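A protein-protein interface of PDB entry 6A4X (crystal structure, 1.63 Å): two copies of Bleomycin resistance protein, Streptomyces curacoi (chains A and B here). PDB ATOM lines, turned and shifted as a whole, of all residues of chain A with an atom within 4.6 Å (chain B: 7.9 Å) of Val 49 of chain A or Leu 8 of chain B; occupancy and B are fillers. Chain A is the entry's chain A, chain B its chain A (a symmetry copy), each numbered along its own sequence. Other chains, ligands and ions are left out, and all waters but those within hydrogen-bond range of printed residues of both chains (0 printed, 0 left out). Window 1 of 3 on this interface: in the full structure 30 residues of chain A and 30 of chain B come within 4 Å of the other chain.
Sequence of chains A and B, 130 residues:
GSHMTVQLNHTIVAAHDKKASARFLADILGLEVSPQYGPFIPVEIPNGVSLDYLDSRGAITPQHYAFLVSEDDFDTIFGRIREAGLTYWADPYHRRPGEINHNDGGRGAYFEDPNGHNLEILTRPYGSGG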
ATOM      1  N   LEU A   8      13.088 -14.164  16.049  1.00  0.00           N
ATOM      2  CA  LEU A   8      13.304 -12.901  16.739  1.00  0.00           C
ATOM      3  C   LEU A   8      13.629 -13.206  18.192  1.00  0.00           C
ATOM      4  O   LEU A   8      12.802 -13.770  18.918  1.00  0.00           O
ATOM      5  CB  LEU A   8      12.081 -11.990  16.633  1.00  0.00           C
ATOM      6  CG  LEU A   8      12.243 -10.659  17.364  1.00  0.00           C
ATOM      7  CD1 LEU A   8      13.311  -9.785  16.690  1.00  0.00           C
ATOM      8  CD2 LEU A   8      10.917  -9.892  17.498  1.00  0.00           C
ATOM      9  N   ASN A   9      14.836 -12.841  18.617  1.00  0.00           N
ATOM     10  CA  ASN A   9      15.346 -13.201  19.935  1.00  0.00           C
ATOM     11  C   ASN A   9      15.164 -12.107  20.980  1.00  0.00           C
ATOM     12  O   ASN A   9      14.876 -12.418  22.140  1.00  0.00           O
ATOM     13  CB  ASN A   9      16.834 -13.567  19.836  1.00  0.00           C
ATOM     14  CG  ASN A   9      17.402 -14.056  21.151  1.00  0.00           C
ATOM     15  OD1 ASN A   9      17.239 -15.231  21.515  1.00  0.00           O
ATOM     16  ND2 ASN A   9      18.067 -13.163  21.885  1.00  0.00           N
ATOM     17  N   HIS A  10      15.366 -10.838  20.624  1.00  0.00           N
ATOM     18  CA  HIS A  10      15.075  -9.768  21.575  1.00  0.00           C
ATOM     19  C   HIS A  10      14.931  -8.437  20.848  1.00  0.00           C
ATOM     20  O   HIS A  10      15.350  -8.276  19.700  1.00  0.00           O
ATOM     21  CB  HIS A  10      16.128  -9.679  22.702  1.00  0.00           C
ATOM     22  CG  HIS A  10      17.531  -9.376  22.250  1.00  0.00           C
ATOM     23  ND1 HIS A  10      18.431 -10.358  21.890  1.00  0.00           N
ATOM     24  CD2 HIS A  10      18.208  -8.205  22.181  1.00  0.00           C
ATOM     25  CE1 HIS A  10      19.594  -9.803  21.595  1.00  0.00           C
ATOM     26  NE2 HIS A  10      19.483  -8.495  21.752  1.00  0.00           N
ATOM     27  N   VAL A  43      12.504  -9.387  29.918  1.00  0.00           N
ATOM     28  CA  VAL A  43      11.273 -10.130  30.193  1.00  0.00           C
ATOM     29  C   VAL A  43      11.107 -11.150  29.074  1.00  0.00           C
ATOM     30  O   VAL A  43      10.867 -10.777  27.918  1.00  0.00           O
ATOM     31  CB  VAL A  43      10.039  -9.219  30.296  1.00  0.00           C
ATOM     32  CG1 VAL A  43       8.803 -10.057  30.575  1.00  0.00           C
ATOM     33  CG2 VAL A  43      10.226  -8.186  31.397  1.00  0.00           C
ATOM     34  N   GLU A  44      11.232 -12.436  29.409  1.00  0.00           N
ATOM     35  CA  GLU A  44      11.143 -13.491  28.408  1.00  0.00           C
ATOM     36  C   GLU A  44       9.682 -13.780  28.076  1.00  0.00           C
ATOM     37  O   GLU A  44       8.886 -14.112  28.965  1.00  0.00           O
ATOM     38  CB  GLU A  44      11.840 -14.761  28.899  1.00  0.00           C
ATOM     39  CG  GLU A  44      13.337 -14.611  29.116  1.00  0.00           C
ATOM     40  CD  GLU A  44      14.144 -14.625  27.817  1.00  0.00           C
ATOM     41  OE1 GLU A  44      13.566 -14.907  26.742  1.00  0.00           O
ATOM     42  OE2 GLU A  44      15.369 -14.363  27.882  1.00  0.00           O
ATOM     43  N   ILE A  45       9.335 -13.665  26.800  1.00  0.00           N
ATOM     44  CA  ILE A  45       8.005 -14.027  26.324  1.00  0.00           C
ATOM     45  C   ILE A  45       8.086 -15.472  25.848  1.00  0.00           C
ATOM     46  O   ILE A  45       9.105 -15.874  25.271  1.00  0.00           O
ATOM     47  CB  ILE A  45       7.511 -13.081  25.214  1.00  0.00           C
ATOM     48  CG1 ILE A  45       7.850 -11.608  25.516  1.00  0.00           C
ATOM     49  CG2 ILE A  45       6.006 -13.241  25.012  1.00  0.00           C
ATOM     50  CD1 ILE A  45       7.303 -11.061  26.841  1.00  0.00           C
ATOM     51  N   ASN A  47       7.342 -17.313  23.400  1.00  0.00           N
ATOM     52  CA  ASN A  47       7.690 -17.751  22.051  1.00  0.00           C
ATOM     53  C   ASN A  47       9.121 -17.396  21.652  1.00  0.00           C
ATOM     54  O   ASN A  47       9.430 -17.353  20.461  1.00  0.00           O
ATOM     55  CB  ASN A  47       6.690 -17.245  20.997  1.00  0.00           C
ATOM     56  CG  ASN A  47       6.541 -15.744  20.946  1.00  0.00           C
ATOM     57  OD1 ASN A  47       6.559 -15.054  21.960  1.00  0.00           O
ATOM     58  ND2 ASN A  47       6.346 -15.232  19.735  1.00  0.00           N
ATOM     59  N   GLY A  48      10.003 -17.184  22.617  1.00  0.00           N
ATOM     60  CA  GLY A  48      11.430 -17.148  22.338  1.00  0.00           C
ATOM     61  C   GLY A  48      12.015 -15.770  22.162  1.00  0.00           C
ATOM     62  O   GLY A  48      13.180 -15.658  21.770  1.00  0.00           O
ATOM     63  N   VAL A  49      11.254 -14.723  22.448  1.00  0.00           N
ATOM     64  CA  VAL A  49      11.723 -13.350  22.316  1.00  0.00           C
ATOM     65  C   VAL A  49      11.680 -12.709  23.696  1.00  0.00           C
ATOM     66  O   VAL A  49      10.761 -12.972  24.475  1.00  0.00           O
ATOM     67  CB  VAL A  49      10.874 -12.560  21.296  1.00  0.00           C
ATOM     68  CG1 VAL A  49       9.421 -12.532  21.703  1.00  0.00           C
ATOM     69  CG2 VAL A  49      11.407 -11.136  21.131  1.00  0.00           C
ATOM     70  N   SER A  50      12.695 -11.909  24.028  1.00  0.00           N
ATOM     71  CA  SER A  50      12.645 -11.131  25.259  1.00  0.00           C
ATOM     72  C   SER A  50      12.521  -9.649  24.938  1.00  0.00           C
ATOM     73  O   SER A  50      13.060  -9.169  23.937  1.00  0.00           O
ATOM     74  CB  SER A  50      13.864 -11.375  26.155  1.00  0.00           C
ATOM     75  OG  SER A  50      15.040 -10.891  25.567  1.00  0.00           O
ATOM     76  N   LEU A  51      11.775  -8.936  25.772  1.00  0.00           N
ATOM     77  CA  LEU A  51      11.720  -7.476  25.730  1.00  0.00           C
ATOM     78  C   LEU A  51      12.729  -6.992  26.762  1.00  0.00           C
ATOM     79  O   LEU A  51      12.590  -7.286  27.953  1.00  0.00           O
ATOM     80  CB  LEU A  51      10.308  -6.969  26.033  1.00  0.00           C
ATOM     81  CG  LEU A  51       9.434  -6.724  24.793  1.00  0.00           C
ATOM     82  CD1 LEU A  51       9.293  -7.990  23.984  1.00  0.00           C
ATOM     83  CD2 LEU A  51       8.047  -6.200  25.182  1.00  0.00           C
ATOM     84  N   TYR A  65       3.703  -3.100  21.072  1.00  0.00           N
ATOM     85  CA  TYR A  65       3.978  -4.503  21.358  1.00  0.00           C
ATOM     86  C   TYR A  65       2.641  -5.197  21.550  1.00  0.00           C
ATOM     87  O   TYR A  65       1.895  -4.860  22.475  1.00  0.00           O
ATOM     88  CB  TYR A  65       4.863  -4.658  22.596  1.00  0.00           C
ATOM     89  CG  TYR A  65       6.152  -3.865  22.513  1.00  0.00           C
ATOM     90  CD1 TYR A  65       7.156  -4.237  21.630  1.00  0.00           C
ATOM     91  CD2 TYR A  65       6.349  -2.727  23.299  1.00  0.00           C
ATOM     92  CE1 TYR A  65       8.335  -3.504  21.538  1.00  0.00           C
ATOM     93  CE2 TYR A  65       7.520  -1.986  23.215  1.00  0.00           C
ATOM     94  CZ  TYR A  65       8.515  -2.385  22.333  1.00  0.00           C
ATOM     95  OH  TYR A  65       9.687  -1.667  22.227  1.00  0.00           O
ATOM     96  N   ALA A  66       2.343  -6.153  20.680  1.00  0.00           N
ATOM     97  CA  ALA A  66       1.055  -6.840  20.689  1.00  0.00           C
ATOM     98  C   ALA A  66       1.260  -8.299  21.049  1.00  0.00           C
ATOM     99  O   ALA A  66       2.114  -8.967  20.463  1.00  0.00           O
ATOM    100  CB  ALA A  66       0.374  -6.740  19.333  1.00  0.00           C
ATOM    101  N   PHE A  67       0.459  -8.794  21.984  1.00  0.00           N
ATOM    102  CA  PHE A  67       0.622 -10.134  22.525  1.00  0.00           C
ATOM    103  C   PHE A  67      -0.606 -10.957  22.192  1.00  0.00           C
ATOM    104  O   PHE A  67      -1.730 -10.535  22.478  1.00  0.00           O
ATOM    105  CB  PHE A  67       0.839 -10.086  24.041  1.00  0.00           C
ATOM    106  CG  PHE A  67       2.074  -9.335  24.425  1.00  0.00           C
ATOM    107  CD1 PHE A  67       3.294  -9.991  24.518  1.00  0.00           C
ATOM    108  CD2 PHE A  67       2.024  -7.972  24.638  1.00  0.00           C
ATOM    109  CE1 PHE A  67       4.446  -9.299  24.840  1.00  0.00           C
ATOM    110  CE2 PHE A  67       3.190  -7.258  24.964  1.00  0.00           C
ATOM    111  CZ  PHE A  67       4.400  -7.931  25.064  1.00  0.00           C
ATOM    112  N   THR B   5       0.405 -19.173  27.971  1.00  0.00           N
ATOM    113  CA  THR B   5       0.918 -19.445  26.627  1.00  0.00           C
ATOM    114  C   THR B   5       1.060 -18.172  25.790  1.00  0.00           C
ATOM    115  O   THR B   5       0.978 -18.209  24.559  1.00  0.00           O
ATOM    116  CB  THR B   5       0.007 -20.456  25.925  1.00  0.00           C
ATOM    117  OG1 THR B   5       0.367 -20.561  24.543  1.00  0.00           O
ATOM    118  CG2 THR B   5      -1.465 -20.044  26.045  1.00  0.00           C
ATOM    119  N   VAL B   6       1.295 -17.050  26.471  1.00  0.00           N
ATOM    120  CA  VAL B   6       1.427 -15.737  25.846  1.00  0.00           C
ATOM    121  C   VAL B   6       2.492 -15.750  24.757  1.00  0.00           C
ATOM    122  O   VAL B   6       3.557 -16.352  24.917  1.00  0.00           O
ATOM    123  CB  VAL B   6       1.766 -14.719  26.950  1.00  0.00           C
ATOM    124  CG1 VAL B   6       2.056 -13.346  26.365  1.00  0.00           C
ATOM    125  CG2 VAL B   6       0.642 -14.674  27.989  1.00  0.00           C
ATOM    126  N   GLN B   7       2.224 -15.055  23.645  1.00  0.00           N
ATOM    127  CA  GLN B   7       3.219 -14.869  22.593  1.00  0.00           C
ATOM    128  C   GLN B   7       3.307 -13.401  22.228  1.00  0.00           C
ATOM    129  O   GLN B   7       2.282 -12.712  22.186  1.00  0.00           O
ATOM    130  CB  GLN B   7       2.871 -15.645  21.324  1.00  0.00           C
ATOM    131  CG  GLN B   7       2.636 -17.122  21.524  1.00  0.00           C
ATOM    132  CD  GLN B   7       2.151 -17.799  20.261  1.00  0.00           C
ATOM    133  OE1 GLN B   7       2.028 -17.171  19.208  1.00  0.00           O
ATOM    134  NE2 GLN B   7       1.855 -19.090  20.364  1.00  0.00           N
ATOM    135  N   LEU B   8       4.528 -12.926  21.953  1.00  0.00           N
ATOM    136  CA  LEU B   8       4.662 -11.664  21.240  1.00  0.00           C
ATOM    137  C   LEU B   8       4.263 -11.894  19.792  1.00  0.00           C
ATOM    138  O   LEU B   8       4.904 -12.674  19.078  1.00  0.00           O
ATOM    139  CB  LEU B   8       6.087 -11.118  21.333  1.00  0.00           C
ATOM    140  CG  LEU B   8       6.291  -9.806  20.579  1.00  0.00           C
ATOM    141  CD1 LEU B   8       5.502  -8.663  21.235  1.00  0.00           C
ATOM    142  CD2 LEU B   8       7.775  -9.431  20.435  1.00  0.00           C
ATOM    143  N   ASN B   9       3.199 -11.222  19.358  1.00  0.00           N
ATOM    144  CA  ASN B   9       2.607 -11.453  18.045  1.00  0.00           C
ATOM    145  C   ASN B   9       3.077 -10.468  16.982  1.00  0.00           C
ATOM    146  O   ASN B   9       3.267 -10.865  15.829  1.00  0.00           O
ATOM    147  CB  ASN B   9       1.076 -11.399  18.147  1.00  0.00           C
ATOM    148  CG  ASN B   9       0.393 -11.738  16.839  1.00  0.00           C
ATOM    149  OD1 ASN B   9       0.230 -12.918  16.497  1.00  0.00           O
ATOM    150  ND2 ASN B   9      -0.006 -10.711  16.089  1.00  0.00           N
ATOM    151  N   HIS B  10       3.229  -9.185  17.315  1.00  0.00           N
ATOM    152  CA  HIS B  10       3.797  -8.252  16.346  1.00  0.00           C
ATOM    153  C   HIS B  10       4.300  -6.997  17.051  1.00  0.00           C
ATOM    154  O   HIS B  10       3.943  -6.709  18.195  1.00  0.00           O
ATOM    155  CB  HIS B  10       2.806  -7.900  15.216  1.00  0.00           C
ATOM    156  CG  HIS B  10       1.539  -7.218  15.659  1.00  0.00           C
ATOM    157  ND1 HIS B  10       0.406  -7.913  16.034  1.00  0.00           N
ATOM    158  CD2 HIS B  10       1.206  -5.907  15.706  1.00  0.00           C
ATOM    159  CE1 HIS B  10      -0.561  -7.057  16.317  1.00  0.00           C
ATOM    160  NE2 HIS B  10      -0.099  -5.831  16.137  1.00  0.00           N
ATOM    161  N   THR B  11       5.203  -6.296  16.362  1.00  0.00           N
ATOM    162  CA  THR B  11       5.617  -4.946  16.720  1.00  0.00           C
ATOM    163  C   THR B  11       5.640  -4.138  15.432  1.00  0.00           C
ATOM    164  O   THR B  11       5.668  -4.701  14.337  1.00  0.00           O
ATOM    165  CB  THR B  11       6.982  -4.918  17.452  1.00  0.00           C
ATOM    166  OG1 THR B  11       7.232  -3.594  17.956  1.00  0.00           O
ATOM    167  CG2 THR B  11       8.113  -5.349  16.527  1.00  0.00           C
ATOM    168  N   ILE B  45       8.249 -13.652  11.204  1.00  0.00           N
ATOM    169  CA  ILE B  45       9.432 -14.354  11.689  1.00  0.00           C
ATOM    170  C   ILE B  45       8.962 -15.714  12.190  1.00  0.00           C
ATOM    171  O   ILE B  45       7.874 -15.814  12.772  1.00  0.00           O
ATOM    172  CB  ILE B  45      10.167 -13.558  12.784  1.00  0.00           C
ATOM    173  CG1 ILE B  45      10.241 -12.055  12.456  1.00  0.00           C
ATOM    174  CG2 ILE B  45      11.572 -14.118  12.992  1.00  0.00           C
ATOM    175  CD1 ILE B  45      10.913 -11.700  11.123  1.00  0.00           C
ATOM    176  N   ASN B  47       9.184 -17.645  14.672  1.00  0.00           N
ATOM    177  CA  ASN B  47       8.733 -17.949  16.028  1.00  0.00           C
ATOM    178  C   ASN B  47       7.453 -17.212  16.416  1.00  0.00           C
ATOM    179  O   ASN B  47       7.170 -17.065  17.606  1.00  0.00           O
ATOM    180  CB  ASN B  47       9.835 -17.715  17.075  1.00  0.00           C
ATOM    181  CG  ASN B  47      10.387 -16.311  17.100  1.00  0.00           C
ATOM    182  OD1 ASN B  47      10.554 -15.660  16.074  1.00  0.00           O
ATOM    183  ND2 ASN B  47      10.717 -15.850  18.303  1.00  0.00           N
ATOM    184  N   GLY B  48       6.660 -16.784  15.446  1.00  0.00           N
ATOM    185  CA  GLY B  48       5.297 -16.357  15.720  1.00  0.00           C
ATOM    186  C   GLY B  48       5.109 -14.869  15.871  1.00  0.00           C
ATOM    187  O   GLY B  48       4.019 -14.437  16.258  1.00  0.00           O
ATOM    188  N   VAL B  49       6.126 -14.073  15.569  1.00  0.00           N
ATOM    189  CA  VAL B  49       6.048 -12.623  15.676  1.00  0.00           C
ATOM    190  C   VAL B  49       6.259 -12.041  14.286  1.00  0.00           C
ATOM    191  O   VAL B  49       7.071 -12.558  13.513  1.00  0.00           O
ATOM    192  CB  VAL B  49       7.082 -12.076  16.684  1.00  0.00           C
ATOM    193  CG1 VAL B  49       8.487 -12.451  16.281  1.00  0.00           C
ATOM    194  CG2 VAL B  49       6.957 -10.557  16.824  1.00  0.00           C
ATOM    195  N   SER B  50       5.500 -11.001  13.937  1.00  0.00           N
ATOM    196  CA  SER B  50       5.757 -10.288  12.693  1.00  0.00           C
ATOM    197  C   SER B  50       6.280  -8.890  12.989  1.00  0.00           C
ATOM    198  O   SER B  50       5.894  -8.264  13.979  1.00  0.00           O
ATOM    199  CB  SER B  50       4.515 -10.207  11.799  1.00  0.00           C
ATOM    200  OG  SER B  50       3.516  -9.411  12.375  1.00  0.00           O
ATOM    201  N   LEU B  51       7.190  -8.421  12.144  1.00  0.00           N
ATOM    202  CA  LEU B  51       7.639  -7.031  12.160  1.00  0.00           C
ATOM    203  C   LEU B  51       6.798  -6.309  11.118  1.00  0.00           C
ATOM    204  O   LEU B  51       6.848  -6.650   9.933  1.00  0.00           O
ATOM    205  CB  LEU B  51       9.135  -6.932  11.852  1.00  0.00           C
ATOM    206  CG  LEU B  51      10.046  -6.912  13.090  1.00  0.00           C
ATOM    207  CD1 LEU B  51       9.839  -8.154  13.921  1.00  0.00           C
ATOM    208  CD2 LEU B  51      11.522  -6.792  12.695  1.00  0.00           C
ATOM    209  N   ALA B  66      17.035  -8.219  17.210  1.00  0.00           N
ATOM    210  CA  ALA B  66      18.087  -9.230  17.215  1.00  0.00           C
ATOM    211  C   ALA B  66      17.493 -10.584  16.881  1.00  0.00           C
ATOM    212  O   ALA B  66      16.490 -10.986  17.476  1.00  0.00           O
ATOM    213  CB  ALA B  66      18.773  -9.295  18.571  1.00  0.00           C
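The backbone NH (N) of Leu 8 of chain A lies within hydrogen-bond range of the side-chain amide oxygen (OD1) of Asn 47 of chain B (2.9 Å). The backbone NH of Asn 9 of chain A lies within hydrogen-bond range of the backbone carbonyl oxygen of Ala 66 of chain B. O of His 10 of chain A sits at hydrogen-bond distance from N of Ala 66 of chain B (3.0 Å). The side-chain amide oxygen of Asn 47 of chain A lies within hydrogen-bond range of the backbone NH of Leu 8 of chain B, 2.9 Å away. The backbone carbonyl oxygen (O) of Asn 47 of chain A is in hydrogen-bond range of the side-chain amide nitrogen (ND2) of Asn 47 of chain B (2.9 Å). The backbone NH (N) of Asn 9 of chain B sits at hydrogen-bond distance from the backbone carbonyl oxygen (O) of Ala 66 of chain A (2.7 Å). N of Ala 66 of chain A lies within hydrogen-bond range of O of His 10 of chain B.
A ring nitrogen (ND1) of His 10 of chain A sits at hydrogen-bond distance from the side-chain amide nitrogen (ND2) of Asn 9 of chain A, 2.8 Å away. N of Ser 50 of chain A sits at hydrogen-bond distance from O of Asn 9 of chain A. The side-chain amide nitrogen of Asn 9 of chain B lies within hydrogen-bond range of a ring nitrogen (ND1) of His 10 of chain B (2.8 Å). O of Asn 9 of chain B sits at hydrogen-bond distance from N of Ser 50 of chain B (2.9 Å). O of Ser 50 of chain B is in hydrogen-bond range of N of Thr 11 of chain B.
Among the printed residues, pairs that only touch across the chains: Phe 67 of chain A with Gln 7 of chain B, Asn 47 of chain A with Gln 7 of chain B, Ile 45 of chain A with Leu 8 of chain B, Leu 8 of chain A with Ile 45 of chain B, Leu 8 of chain A with Ala 66 of chain B, Ala 66 of chain A with Leu 8 of chain B, Val 49 of chain A with Leu 8 of chain B, Leu 8 of chain A with Val 49 of chain B, Tyr 65 of chain A with Thr 11 of chain B, Phe 67 of chain A with Leu 8 of chain B, Tyr 65 of chain A with His 10 of chain B, Ile 45 of chain A with Gln 7 of chain B and Ile 45 of chain A with Val 6 of chain B.
Printed residues of chain B within 4 Å of Leu 8 of chain A: Ile 45, Asn 47, Val 49 and Ala 66. Of the printed residues of chain B, Ile 45 of chain A touches Val 6 (3.96 Å), Gln 7 (3.9 Å) and Leu 8 (3.4 Å). No residue of chain B comes within 4 Å of Gly 48 of chain A. Val 49 of chain A touches one residue of chain B. Of the printed residues of chain A, Leu 8 of chain B touches Ile 45 (3.4 Å), Asn 47 (2.9 Å), Val 49 (3.6 Å), Ala 66 (3.5 Å) and Phe 67 (3.8 Å). Of the printed residues of chain A, Ile 45 of chain B touches Leu 8. The nearest residue of chain B that does not touch Val 49 of chain A is Asn 47 of chain B (4.3 Å). The nearest printed residue of chain B that does not touch Asn 47 of chain A is Gly 48 of chain B (4.1 Å).
Printed residues of chain A that touch a printed residue of chain B: Leu 8, Asn 9, His 10, Ile 45, Asn 47, Val 49, Tyr 65, Ala 66 and Phe 67. Hydrophobic or aromatic side chains of chain A within 4 Å of the printed part of chain B: Leu 8, His 10, Ile 45, Val 49, Tyr 65, Ala 66 and Phe 67. Printed residues of chain B that touch a printed residue of chain A: Val 6, Gln 7, Leu 8, Asn 9, His 10, Thr 11, Ile 45, Asn 47, Val 49 and Ala 66. Among the printed residues, no Asp or Glu carboxylate lies within 4 Å of a Lys or Arg side-chain nitrogen of the other chain.
Leu 8 of chain A touches Val 49 of chain B, and with the chains exchanged Val 49 of chain A touches Leu 8 of chain B. Leu 8 of chain A touches Ala 66 of chain B, and with the chains exchanged Ala 66 of chain A touches Leu 8 of chain B. Asn 9 of chain A touches Ala 66 of chain B, and with the chains exchanged Ala 66 of chain A touches Asn 9 of chain B. His 10 of chain A touches Ala 66 of chain B, and with the chains exchanged Ala 66 of chain A touches His 10 of chain B. Of the 20 pairs that touch across the chains among the printed residues, 13 have their exchanged pair printed and touching as well.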
